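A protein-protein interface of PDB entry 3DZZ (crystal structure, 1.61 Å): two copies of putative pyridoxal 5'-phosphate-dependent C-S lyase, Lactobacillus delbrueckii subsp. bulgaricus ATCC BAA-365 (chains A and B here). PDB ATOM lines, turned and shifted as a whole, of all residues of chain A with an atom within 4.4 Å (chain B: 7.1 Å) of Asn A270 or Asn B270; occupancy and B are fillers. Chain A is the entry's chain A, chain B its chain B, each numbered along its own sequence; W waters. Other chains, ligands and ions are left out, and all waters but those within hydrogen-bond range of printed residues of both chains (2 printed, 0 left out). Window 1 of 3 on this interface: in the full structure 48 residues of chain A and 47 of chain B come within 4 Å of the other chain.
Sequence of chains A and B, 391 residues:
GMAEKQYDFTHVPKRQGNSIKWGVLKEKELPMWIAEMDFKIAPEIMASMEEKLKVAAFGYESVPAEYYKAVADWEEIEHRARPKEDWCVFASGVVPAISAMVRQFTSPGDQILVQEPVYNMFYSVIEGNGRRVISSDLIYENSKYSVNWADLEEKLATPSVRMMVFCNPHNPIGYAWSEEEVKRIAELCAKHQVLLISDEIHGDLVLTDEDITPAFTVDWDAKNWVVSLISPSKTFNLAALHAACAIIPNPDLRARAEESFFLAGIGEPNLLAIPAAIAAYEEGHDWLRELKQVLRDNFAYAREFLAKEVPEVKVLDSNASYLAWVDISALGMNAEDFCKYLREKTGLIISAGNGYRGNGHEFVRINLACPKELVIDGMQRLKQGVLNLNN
Water W2 bridges OE1 of Glu B268 and NE2 of His A242.
Water W1 lies within hydrogen-bond range of a ring nitrogen (ND1) of His A242 (3.2 Å), the side-chain amide nitrogen (ND2) of Asn A270 (3.2 Å), the side-chain amide nitrogen (ND2) of Asn B270 (3.3 Å) and a ring nitrogen (ND1) of His B242 (3.5 Å).
Asn A270 touches three residues of chain B.
Printed residues of chain B within 4 Å of Ala A240: Gly B59 (3.3 Å), Asn B270 (3.2 Å) and Leu B271 (2.9 Å).
Printed residues of chain B within 4 Å of Leu A272: Leu B272 (3.8 Å).
Of the printed residues of chain B, Pro A269 touches His B242 (3.6 Å).
The nearest printed residue of chain B that does not touch Pro A269 is Ala B240 (4.3 Å).
Among the printed residues, pairs that only touch across the chains: His A242 with Glu B268, Asn A270 with Ala B240, Ala A240 with Asn B270, Ala A240 with Gly B59, Glu A268 with His B242, His A242 with Asn B270, Asn A270 with His B242, His A242 with Pro B269, Pro A269 with His B242, Asn A270 with Asn B270, Leu A272 with Leu B272, Leu A271 with Leu B272 and Leu A241 with Leu B271.
Printed residues of chain A that touch a printed residue of chain B: Glu A61, Ala A240, Leu A241, His A242, Glu A268, Pro A269, Asn A270, Leu A271 and Leu A272.
Hydrophobic or aromatic side chains of chain A within 4 Å of the printed part of chain B: Ala A240, His A242, Leu A271 and Leu A272.
Hydrophobic or aromatic side chains of chain B within 4 Å of the printed part of chain A: Ala B240, His B242, Leu B271 and Leu B272.
Among the printed residues, 16 pairs touch across the chains.
ND2 of Asn B270 sits at hydrogen-bond distance from O of Leu B241 (2.8 Å).
N of Leu A272 sits at hydrogen-bond distance from OD1 of Asn A270, at 2.9 Å.
The backbone NH (N) of Leu B272 lies within hydrogen-bond range of the side-chain amide oxygen (OD1) of Asn B270, 2.9 Å away.
O of Leu A241 is in hydrogen-bond range of ND2 of Asn A270.
The side-chain amide oxygen (OD1) of Asn B270 is in hydrogen-bond range of the backbone NH (N) of Ala B273.
The side-chain amino group (NZ) of Lys B52 sits at hydrogen-bond distance from the backbone carbonyl oxygen (O) of Leu B271 (2.8 Å).
Leu A241 touches Leu B271, but with the chains exchanged Leu A271 does not touch Leu B241 (4.2 Å).
His A242 touches Pro B269, and with the chains exchanged Pro A269 touches His B242.
His A242 touches Asn B270, and with the chains exchanged Asn A270 touches His B242.
Leu A271 touches Leu B272, but with the chains exchanged Leu A272 does not touch Leu B271 (4.1 Å).
Of the 16 pairs that touch across the chains among the printed residues, 12 have their exchanged pair printed and touching as well.
The backbone carbonyl oxygen of Ala B240 lies within hydrogen-bond range of the backbone NH of Leu A271.
ND2 of Asn B18 lies within hydrogen-bond range of OE1 of Glu A61 (2.8 Å).
The backbone NH (N) of Leu B271 lies within hydrogen-bond range of the backbone carbonyl oxygen (O) of Ala A240, 2.9 Å away.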
ATOM      1  N   GLU A  61      20.046  26.984  10.434  1.00  0.00           N
ATOM      2  CA  GLU A  61      18.602  26.931  10.674  1.00  0.00           C
ATOM      3  C   GLU A  61      18.191  25.542  11.047  1.00  0.00           C
ATOM      4  O   GLU A  61      18.734  24.573  10.553  1.00  0.00           O
ATOM      5  CB  GLU A  61      17.880  27.216   9.365  1.00  0.00           C
ATOM      6  CG  GLU A  61      18.006  28.617   9.004  1.00  0.00           C
ATOM      7  CD  GLU A  61      17.124  29.033   7.853  1.00  0.00           C
ATOM      8  OE1 GLU A  61      15.955  28.511   7.674  1.00  0.00           O
ATOM      9  OE2 GLU A  61      17.611  29.932   7.159  1.00  0.00           O
ATOM     10  N   ALA A 240      15.032  24.058  -7.809  1.00  0.00           N
ATOM     11  CA  ALA A 240      16.286  24.515  -7.160  1.00  0.00           C
ATOM     12  C   ALA A 240      16.116  25.013  -5.723  1.00  0.00           C
ATOM     13  O   ALA A 240      17.057  25.526  -5.122  1.00  0.00           O
ATOM     14  CB  ALA A 240      17.003  25.591  -8.025  1.00  0.00           C
ATOM     15  N   LEU A 241      14.909  24.893  -5.178  1.00  0.00           N
ATOM     16  CA  LEU A 241      14.696  25.286  -3.766  1.00  0.00           C
ATOM     17  C   LEU A 241      15.311  24.287  -2.814  1.00  0.00           C
ATOM     18  O   LEU A 241      15.816  24.656  -1.800  1.00  0.00           O
ATOM     19  CB  LEU A 241      13.234  25.446  -3.426  1.00  0.00           C
ATOM     20  CG  LEU A 241      12.908  25.840  -1.984  1.00  0.00           C
ATOM     21  CD1 LEU A 241      13.486  27.214  -1.633  1.00  0.00           C
ATOM     22  CD2 LEU A 241      11.393  25.792  -1.752  1.00  0.00           C
ATOM     23  N   HIS A 242      15.282  23.012  -3.181  1.00  0.00           N
ATOM     24  CA  HIS A 242      15.848  21.942  -2.326  1.00  0.00           C
ATOM     25  C   HIS A 242      15.127  21.797  -0.962  1.00  0.00           C
ATOM     26  O   HIS A 242      15.736  21.770   0.087  1.00  0.00           O
ATOM     27  CB  HIS A 242      17.384  22.053  -2.186  1.00  0.00           C
ATOM     28  CG  HIS A 242      18.124  21.970  -3.494  1.00  0.00           C
ATOM     29  ND1 HIS A 242      19.474  22.184  -3.583  1.00  0.00           N
ATOM     30  CD2 HIS A 242      17.716  21.653  -4.739  1.00  0.00           C
ATOM     31  CE1 HIS A 242      19.855  22.028  -4.847  1.00  0.00           C
ATOM     32  NE2 HIS A 242      18.811  21.689  -5.565  1.00  0.00           N
ATOM     33  N   GLU A 268      19.547  19.245   6.442  1.00  0.00           N
ATOM     34  CA  GLU A 268      19.493  20.651   6.956  1.00  0.00           C
ATOM     35  C   GLU A 268      19.058  21.591   5.836  1.00  0.00           C
ATOM     36  O   GLU A 268      19.520  21.465   4.697  1.00  0.00           O
ATOM     37  CB  GLU A 268      20.844  21.070   7.510  1.00  0.00           C
ATOM     38  CG  GLU A 268      21.335  20.169   8.636  1.00  0.00           C
ATOM     39  N   PRO A 269      18.147  22.528   6.151  1.00  0.00           N
ATOM     40  CA  PRO A 269      17.660  23.427   5.100  1.00  0.00           C
ATOM     41  C   PRO A 269      18.611  24.536   4.741  1.00  0.00           C
ATOM     42  O   PRO A 269      19.325  25.084   5.606  1.00  0.00           O
ATOM     43  CB  PRO A 269      16.390  24.023   5.688  1.00  0.00           C
ATOM     44  CG  PRO A 269      16.591  23.901   7.165  1.00  0.00           C
ATOM     45  CD  PRO A 269      17.429  22.676   7.416  1.00  0.00           C
ATOM     46  N   ASN A 270      18.578  24.841   3.451  1.00  0.00           N
ATOM     47  CA  ASN A 270      19.200  26.077   3.000  1.00  0.00           C
ATOM     48  C   ASN A 270      18.362  27.288   3.441  1.00  0.00           C
ATOM     49  O   ASN A 270      17.294  27.137   4.044  1.00  0.00           O
ATOM     50  CB  ASN A 270      19.491  26.056   1.474  1.00  0.00           C
ATOM     51  CG  ASN A 270      18.256  26.119   0.645  1.00  0.00           C
ATOM     52  OD1 ASN A 270      17.337  26.893   0.946  1.00  0.00           O
ATOM     53  ND2 ASN A 270      18.183  25.255  -0.378  1.00  0.00           N
ATOM     54  N   LEU A 271      18.880  28.476   3.124  1.00  0.00           N
ATOM     55  CA  LEU A 271      18.323  29.768   3.600  1.00  0.00           C
ATOM     56  C   LEU A 271      16.893  30.102   3.132  1.00  0.00           C
ATOM     57  O   LEU A 271      16.270  30.948   3.746  1.00  0.00           O
ATOM     58  CB  LEU A 271      19.232  30.951   3.228  1.00  0.00           C
ATOM     59  CG  LEU A 271      19.380  31.372   1.763  1.00  0.00           C
ATOM     60  CD1 LEU A 271      20.570  32.253   1.625  1.00  0.00           C
ATOM     61  CD2 LEU A 271      19.574  30.214   0.763  1.00  0.00           C
ATOM     62  N   LEU A 272      16.373  29.396   2.130  1.00  0.00           N
ATOM     63  CA  LEU A 272      15.017  29.644   1.652  1.00  0.00           C
ATOM     64  C   LEU A 272      14.062  28.486   1.813  1.00  0.00           C
ATOM     65  O   LEU A 272      12.844  28.702   1.732  1.00  0.00           O
ATOM     66  CB  LEU A 272      14.967  30.141   0.211  1.00  0.00           C
ATOM     67  CG  LEU A 272      15.597  31.514  -0.104  1.00  0.00           C
ATOM     68  CD1 LEU A 272      15.510  31.875  -1.606  1.00  0.00           C
ATOM     69  CD2 LEU A 272      15.003  32.668   0.727  1.00  0.00           C
ATOM     70  N   ALA A 273      14.597  27.267   1.982  1.00  0.00           N
ATOM     71  CA  ALA A 273      13.773  26.052   1.933  1.00  0.00           C
ATOM     72  C   ALA A 273      12.605  26.144   2.896  1.00  0.00           C
ATOM     73  O   ALA A 273      11.452  25.808   2.511  1.00  0.00           O
ATOM     74  CB  ALA A 273      14.627  24.811   2.204  1.00  0.00           C
ATOM     75  N   ASN B  18      13.519  30.229  13.377  1.00  0.00           N
ATOM     76  CA  ASN B  18      14.143  28.904  13.297  1.00  0.00           C
ATOM     77  C   ASN B  18      15.650  29.015  13.277  1.00  0.00           C
ATOM     78  O   ASN B  18      16.339  28.106  12.929  1.00  0.00           O
ATOM     79  CB  ASN B  18      13.631  28.069  12.127  1.00  0.00           C
ATOM     80  CG  ASN B  18      13.990  28.655  10.790  1.00  0.00           C
ATOM     81  OD1 ASN B  18      14.024  29.893  10.627  1.00  0.00           O
ATOM     82  ND2 ASN B  18      14.295  27.793   9.843  1.00  0.00           N
ATOM     83  N   LYS B  52      18.684  37.638  -8.491  1.00  0.00           N
ATOM     84  CA  LYS B  52      18.299  36.295  -8.827  1.00  0.00           C
ATOM     85  C   LYS B  52      16.814  36.054  -8.562  1.00  0.00           C
ATOM     86  O   LYS B  52      16.147  35.369  -9.381  1.00  0.00           O
ATOM     87  CB  LYS B  52      19.181  35.259  -8.099  1.00  0.00           C
ATOM     88  CG  LYS B  52      18.789  33.795  -8.396  1.00  0.00           C
ATOM     89  CD  LYS B  52      18.882  33.437  -9.910  1.00  0.00           C
ATOM     90  CE  LYS B  52      18.688  31.979 -10.157  1.00  0.00           C
ATOM     91  NZ  LYS B  52      19.837  31.136  -9.588  1.00  0.00           N
ATOM     92  N   GLY B  59      13.956  26.649 -11.633  1.00  0.00           N
ATOM     93  CA  GLY B  59      14.309  25.378 -12.157  1.00  0.00           C
ATOM     94  C   GLY B  59      15.751  25.000 -11.990  1.00  0.00           C
ATOM     95  O   GLY B  59      16.508  25.597 -11.276  1.00  0.00           O
ATOM     96  N   GLU B  61      19.700  24.292 -12.339  1.00  0.00           N
ATOM     97  CA  GLU B  61      20.856  25.153 -12.533  1.00  0.00           C
ATOM     98  C   GLU B  61      22.080  24.331 -12.845  1.00  0.00           C
ATOM     99  O   GLU B  61      22.300  23.259 -12.260  1.00  0.00           O
ATOM    100  CB  GLU B  61      21.244  25.867 -11.246  1.00  0.00           C
ATOM    101  CG  GLU B  61      20.142  26.573 -10.640  1.00  0.00           C
ATOM    102  CD  GLU B  61      20.398  28.015 -10.393  1.00  0.00           C
ATOM    103  OE1 GLU B  61      21.560  28.506 -10.337  1.00  0.00           O
ATOM    104  OE2 GLU B  61      19.383  28.643 -10.217  1.00  0.00           O
ATOM    105  N   PHE B  90      31.853  22.248  -7.849  1.00  0.00           N
ATOM    106  CA  PHE B  90      30.847  22.703  -6.891  1.00  0.00           C
ATOM    107  C   PHE B  90      30.355  21.545  -5.967  1.00  0.00           C
ATOM    108  O   PHE B  90      30.113  20.440  -6.396  1.00  0.00           O
ATOM    109  CB  PHE B  90      29.630  23.229  -7.663  1.00  0.00           C
ATOM    110  CG  PHE B  90      28.504  23.706  -6.775  1.00  0.00           C
ATOM    111  CD1 PHE B  90      28.503  24.974  -6.249  1.00  0.00           C
ATOM    112  CD2 PHE B  90      27.525  22.814  -6.393  1.00  0.00           C
ATOM    113  CE1 PHE B  90      27.486  25.365  -5.385  1.00  0.00           C
ATOM    114  CE2 PHE B  90      26.505  23.205  -5.530  1.00  0.00           C
ATOM    115  CZ  PHE B  90      26.513  24.469  -5.021  1.00  0.00           C
ATOM    116  N   SER B  92      27.393  21.315  -2.443  1.00  0.00           N
ATOM    117  CA  SER B  92      26.457  22.121  -1.638  1.00  0.00           C
ATOM    118  C   SER B  92      26.967  22.460  -0.211  1.00  0.00           C
ATOM    119  O   SER B  92      26.389  23.295   0.522  1.00  0.00           O
ATOM    120  CB  SER B  92      25.090  21.448  -1.640  1.00  0.00           C
ATOM    121  OG  SER B  92      24.528  21.535  -2.956  1.00  0.00           O
ATOM    122  N   ALA B 239      26.230  30.334   6.110  1.00  0.00           N
ATOM    123  CA  ALA B 239      26.172  28.875   6.339  1.00  0.00           C
ATOM    124  C   ALA B 239      24.993  28.218   5.625  1.00  0.00           C
ATOM    125  O   ALA B 239      25.137  27.121   5.088  1.00  0.00           O
ATOM    126  CB  ALA B 239      26.077  28.608   7.836  1.00  0.00           C
ATOM    127  N   ALA B 240      23.877  28.900   5.531  1.00  0.00           N
ATOM    128  CA  ALA B 240      22.703  28.276   4.952  1.00  0.00           C
ATOM    129  C   ALA B 240      22.633  28.465   3.446  1.00  0.00           C
ATOM    130  O   ALA B 240      21.688  28.042   2.824  1.00  0.00           O
ATOM    131  CB  ALA B 240      21.438  28.821   5.656  1.00  0.00           C
ATOM    132  N   LEU B 241      23.639  29.106   2.857  1.00  0.00           N
ATOM    133  CA  LEU B 241      23.665  29.230   1.398  1.00  0.00           C
ATOM    134  C   LEU B 241      23.890  27.896   0.708  1.00  0.00           C
ATOM    135  O   LEU B 241      23.391  27.701  -0.384  1.00  0.00           O
ATOM    136  CB  LEU B 241      24.685  30.248   0.928  1.00  0.00           C
ATOM    137  CG  LEU B 241      24.807  30.454  -0.575  1.00  0.00           C
ATOM    138  CD1 LEU B 241      23.526  31.107  -1.128  1.00  0.00           C
ATOM    139  CD2 LEU B 241      25.980  31.380  -0.908  1.00  0.00           C
ATOM    140  N   HIS B 242      24.646  27.004   1.342  1.00  0.00           N
ATOM    141  CA  HIS B 242      24.979  25.670   0.799  1.00  0.00           C
ATOM    142  C   HIS B 242      25.687  25.815  -0.549  1.00  0.00           C
ATOM    143  O   HIS B 242      25.286  25.265  -1.554  1.00  0.00           O
ATOM    144  CB  HIS B 242      23.729  24.773   0.753  1.00  0.00           C
ATOM    145  CG  HIS B 242      23.174  24.459   2.102  1.00  0.00           C
ATOM    146  ND1 HIS B 242      22.117  23.598   2.286  1.00  0.00           N
ATOM    147  CD2 HIS B 242      23.541  24.875   3.339  1.00  0.00           C
ATOM    148  CE1 HIS B 242      21.857  23.503   3.576  1.00  0.00           C
ATOM    149  NE2 HIS B 242      22.707  24.272   4.242  1.00  0.00           N
ATOM    150  N   ALA B 243      26.780  26.575  -0.525  1.00  0.00           N
ATOM    151  CA  ALA B 243      27.671  26.710  -1.656  1.00  0.00           C
ATOM    152  C   ALA B 243      29.097  26.452  -1.179  1.00  0.00           C
ATOM    153  O   ALA B 243      29.531  27.012  -0.199  1.00  0.00           O
ATOM    154  CB  ALA B 243      27.526  28.059  -2.281  1.00  0.00           C
ATOM    155  N   GLU B 268      24.286  19.703  -7.081  1.00  0.00           N
ATOM    156  CA  GLU B 268      23.429  20.644  -7.876  1.00  0.00           C
ATOM    157  C   GLU B 268      23.202  21.868  -7.034  1.00  0.00           C
ATOM    158  O   GLU B 268      22.799  21.757  -5.887  1.00  0.00           O
ATOM    159  CB  GLU B 268      22.062  20.059  -8.236  1.00  0.00           C
ATOM    160  CG  GLU B 268      22.098  18.839  -9.127  1.00  0.00           C
ATOM    161  CD  GLU B 268      20.694  18.325  -9.521  1.00  0.00           C
ATOM    162  OE1 GLU B 268      19.682  18.977  -9.188  1.00  0.00           O
ATOM    163  OE2 GLU B 268      20.615  17.251 -10.179  1.00  0.00           O
ATOM    164  N   PRO B 269      23.492  23.054  -7.581  1.00  0.00           N
ATOM    165  CA  PRO B 269      23.258  24.225  -6.754  1.00  0.00           C
ATOM    166  C   PRO B 269      21.796  24.521  -6.537  1.00  0.00           C
ATOM    167  O   PRO B 269      20.982  24.357  -7.430  1.00  0.00           O
ATOM    168  CB  PRO B 269      23.788  25.378  -7.594  1.00  0.00           C
ATOM    169  CG  PRO B 269      24.220  24.856  -8.839  1.00  0.00           C
ATOM    170  CD  PRO B 269      24.079  23.372  -8.892  1.00  0.00           C
ATOM    171  N   ASN B 270      21.512  25.060  -5.355  1.00  0.00           N
ATOM    172  CA  ASN B 270      20.239  25.666  -5.099  1.00  0.00           C
ATOM    173  C   ASN B 270      20.133  27.027  -5.795  1.00  0.00           C
ATOM    174  O   ASN B 270      21.060  27.491  -6.415  1.00  0.00           O
ATOM    175  CB  ASN B 270      19.912  25.755  -3.638  1.00  0.00           C
ATOM    176  CG  ASN B 270      20.776  26.789  -2.876  1.00  0.00           C
ATOM    177  OD1 ASN B 270      20.935  27.907  -3.329  1.00  0.00           O
ATOM    178  ND2 ASN B 270      21.355  26.389  -1.715  1.00  0.00           N
ATOM    179  N   LEU B 271      18.971  27.645  -5.702  1.00  0.00           N
ATOM    180  CA  LEU B 271      18.656  28.777  -6.559  1.00  0.00           C
ATOM    181  C   LEU B 271      19.326  30.082  -6.173  1.00  0.00           C
ATOM    182  O   LEU B 271      19.119  31.095  -6.835  1.00  0.00           O
ATOM    183  CB  LEU B 271      17.150  28.994  -6.623  1.00  0.00           C
ATOM    184  CG  LEU B 271      16.585  29.593  -5.335  1.00  0.00           C
ATOM    185  CD1 LEU B 271      16.512  31.105  -5.454  1.00  0.00           C
ATOM    186  CD2 LEU B 271      15.200  29.010  -5.056  1.00  0.00           C
ATOM    187  N   LEU B 272      20.114  30.072  -5.109  1.00  0.00           N
ATOM    188  CA  LEU B 272      20.959  31.265  -4.768  1.00  0.00           C
ATOM    189  C   LEU B 272      22.449  31.026  -4.794  1.00  0.00           C
ATOM    190  O   LEU B 272      23.220  31.957  -4.789  1.00  0.00           O
ATOM    191  CB  LEU B 272      20.588  31.899  -3.418  1.00  0.00           C
ATOM    192  CG  LEU B 272      19.213  32.581  -3.300  1.00  0.00           C
ATOM    193  CD1 LEU B 272      19.044  33.207  -1.885  1.00  0.00           C
ATOM    194  CD2 LEU B 272      19.077  33.650  -4.456  1.00  0.00           C
ATOM    195  N   ALA B 273      22.849  29.758  -4.692  1.00  0.00           N
ATOM    196  CA  ALA B 273      24.232  29.382  -4.450  1.00  0.00           C
ATOM    197  C   ALA B 273      25.191  30.030  -5.461  1.00  0.00           C
ATOM    198  O   ALA B 273      26.249  30.582  -5.117  1.00  0.00           O
ATOM    199  CB  ALA B 273      24.364  27.859  -4.407  1.00  0.00           C
ATOM    200  N   ILE B 274      24.840  29.949  -6.716  1.00  0.00           N
ATOM    201  CA  ILE B 274      25.725  30.437  -7.778  1.00  0.00           C
ATOM    202  C   ILE B 274      25.867  31.945  -7.808  1.00  0.00           C
ATOM    203  O   ILE B 274      26.972  32.461  -7.658  1.00  0.00           O
ATOM    204  CB  ILE B 274      25.341  29.830  -9.164  1.00  0.00           C
ATOM    205  CG1 ILE B 274      25.524  28.299  -9.209  1.00  0.00           C
ATOM    206  CG2 ILE B 274      26.191  30.508 -10.291  1.00  0.00           C
ATOM    207  CD1 ILE B 274      26.825  27.771  -8.680  1.00  0.00           C
ATOM    208  N   PRO B 275      24.760  32.722  -7.949  1.00  0.00           N
ATOM    209  CA  PRO B 275      24.961  34.144  -7.984  1.00  0.00           C
ATOM    210  C   PRO B 275      25.568  34.720  -6.694  1.00  0.00           C
ATOM    211  O   PRO B 275      26.353  35.659  -6.731  1.00  0.00           O
ATOM    212  CB  PRO B 275      23.532  34.706  -8.249  1.00  0.00           C
ATOM    213  CG  PRO B 275      22.649  33.607  -7.851  1.00  0.00           C
ATOM    214  CD  PRO B 275      23.372  32.365  -8.242  1.00  0.00           C
HETATM  215  O   HOH W   1      20.723  23.303  -0.906  1.00  0.00           O
HETATM  216  O   HOH W   2      18.352  21.070  -8.202  1.00  0.00           O
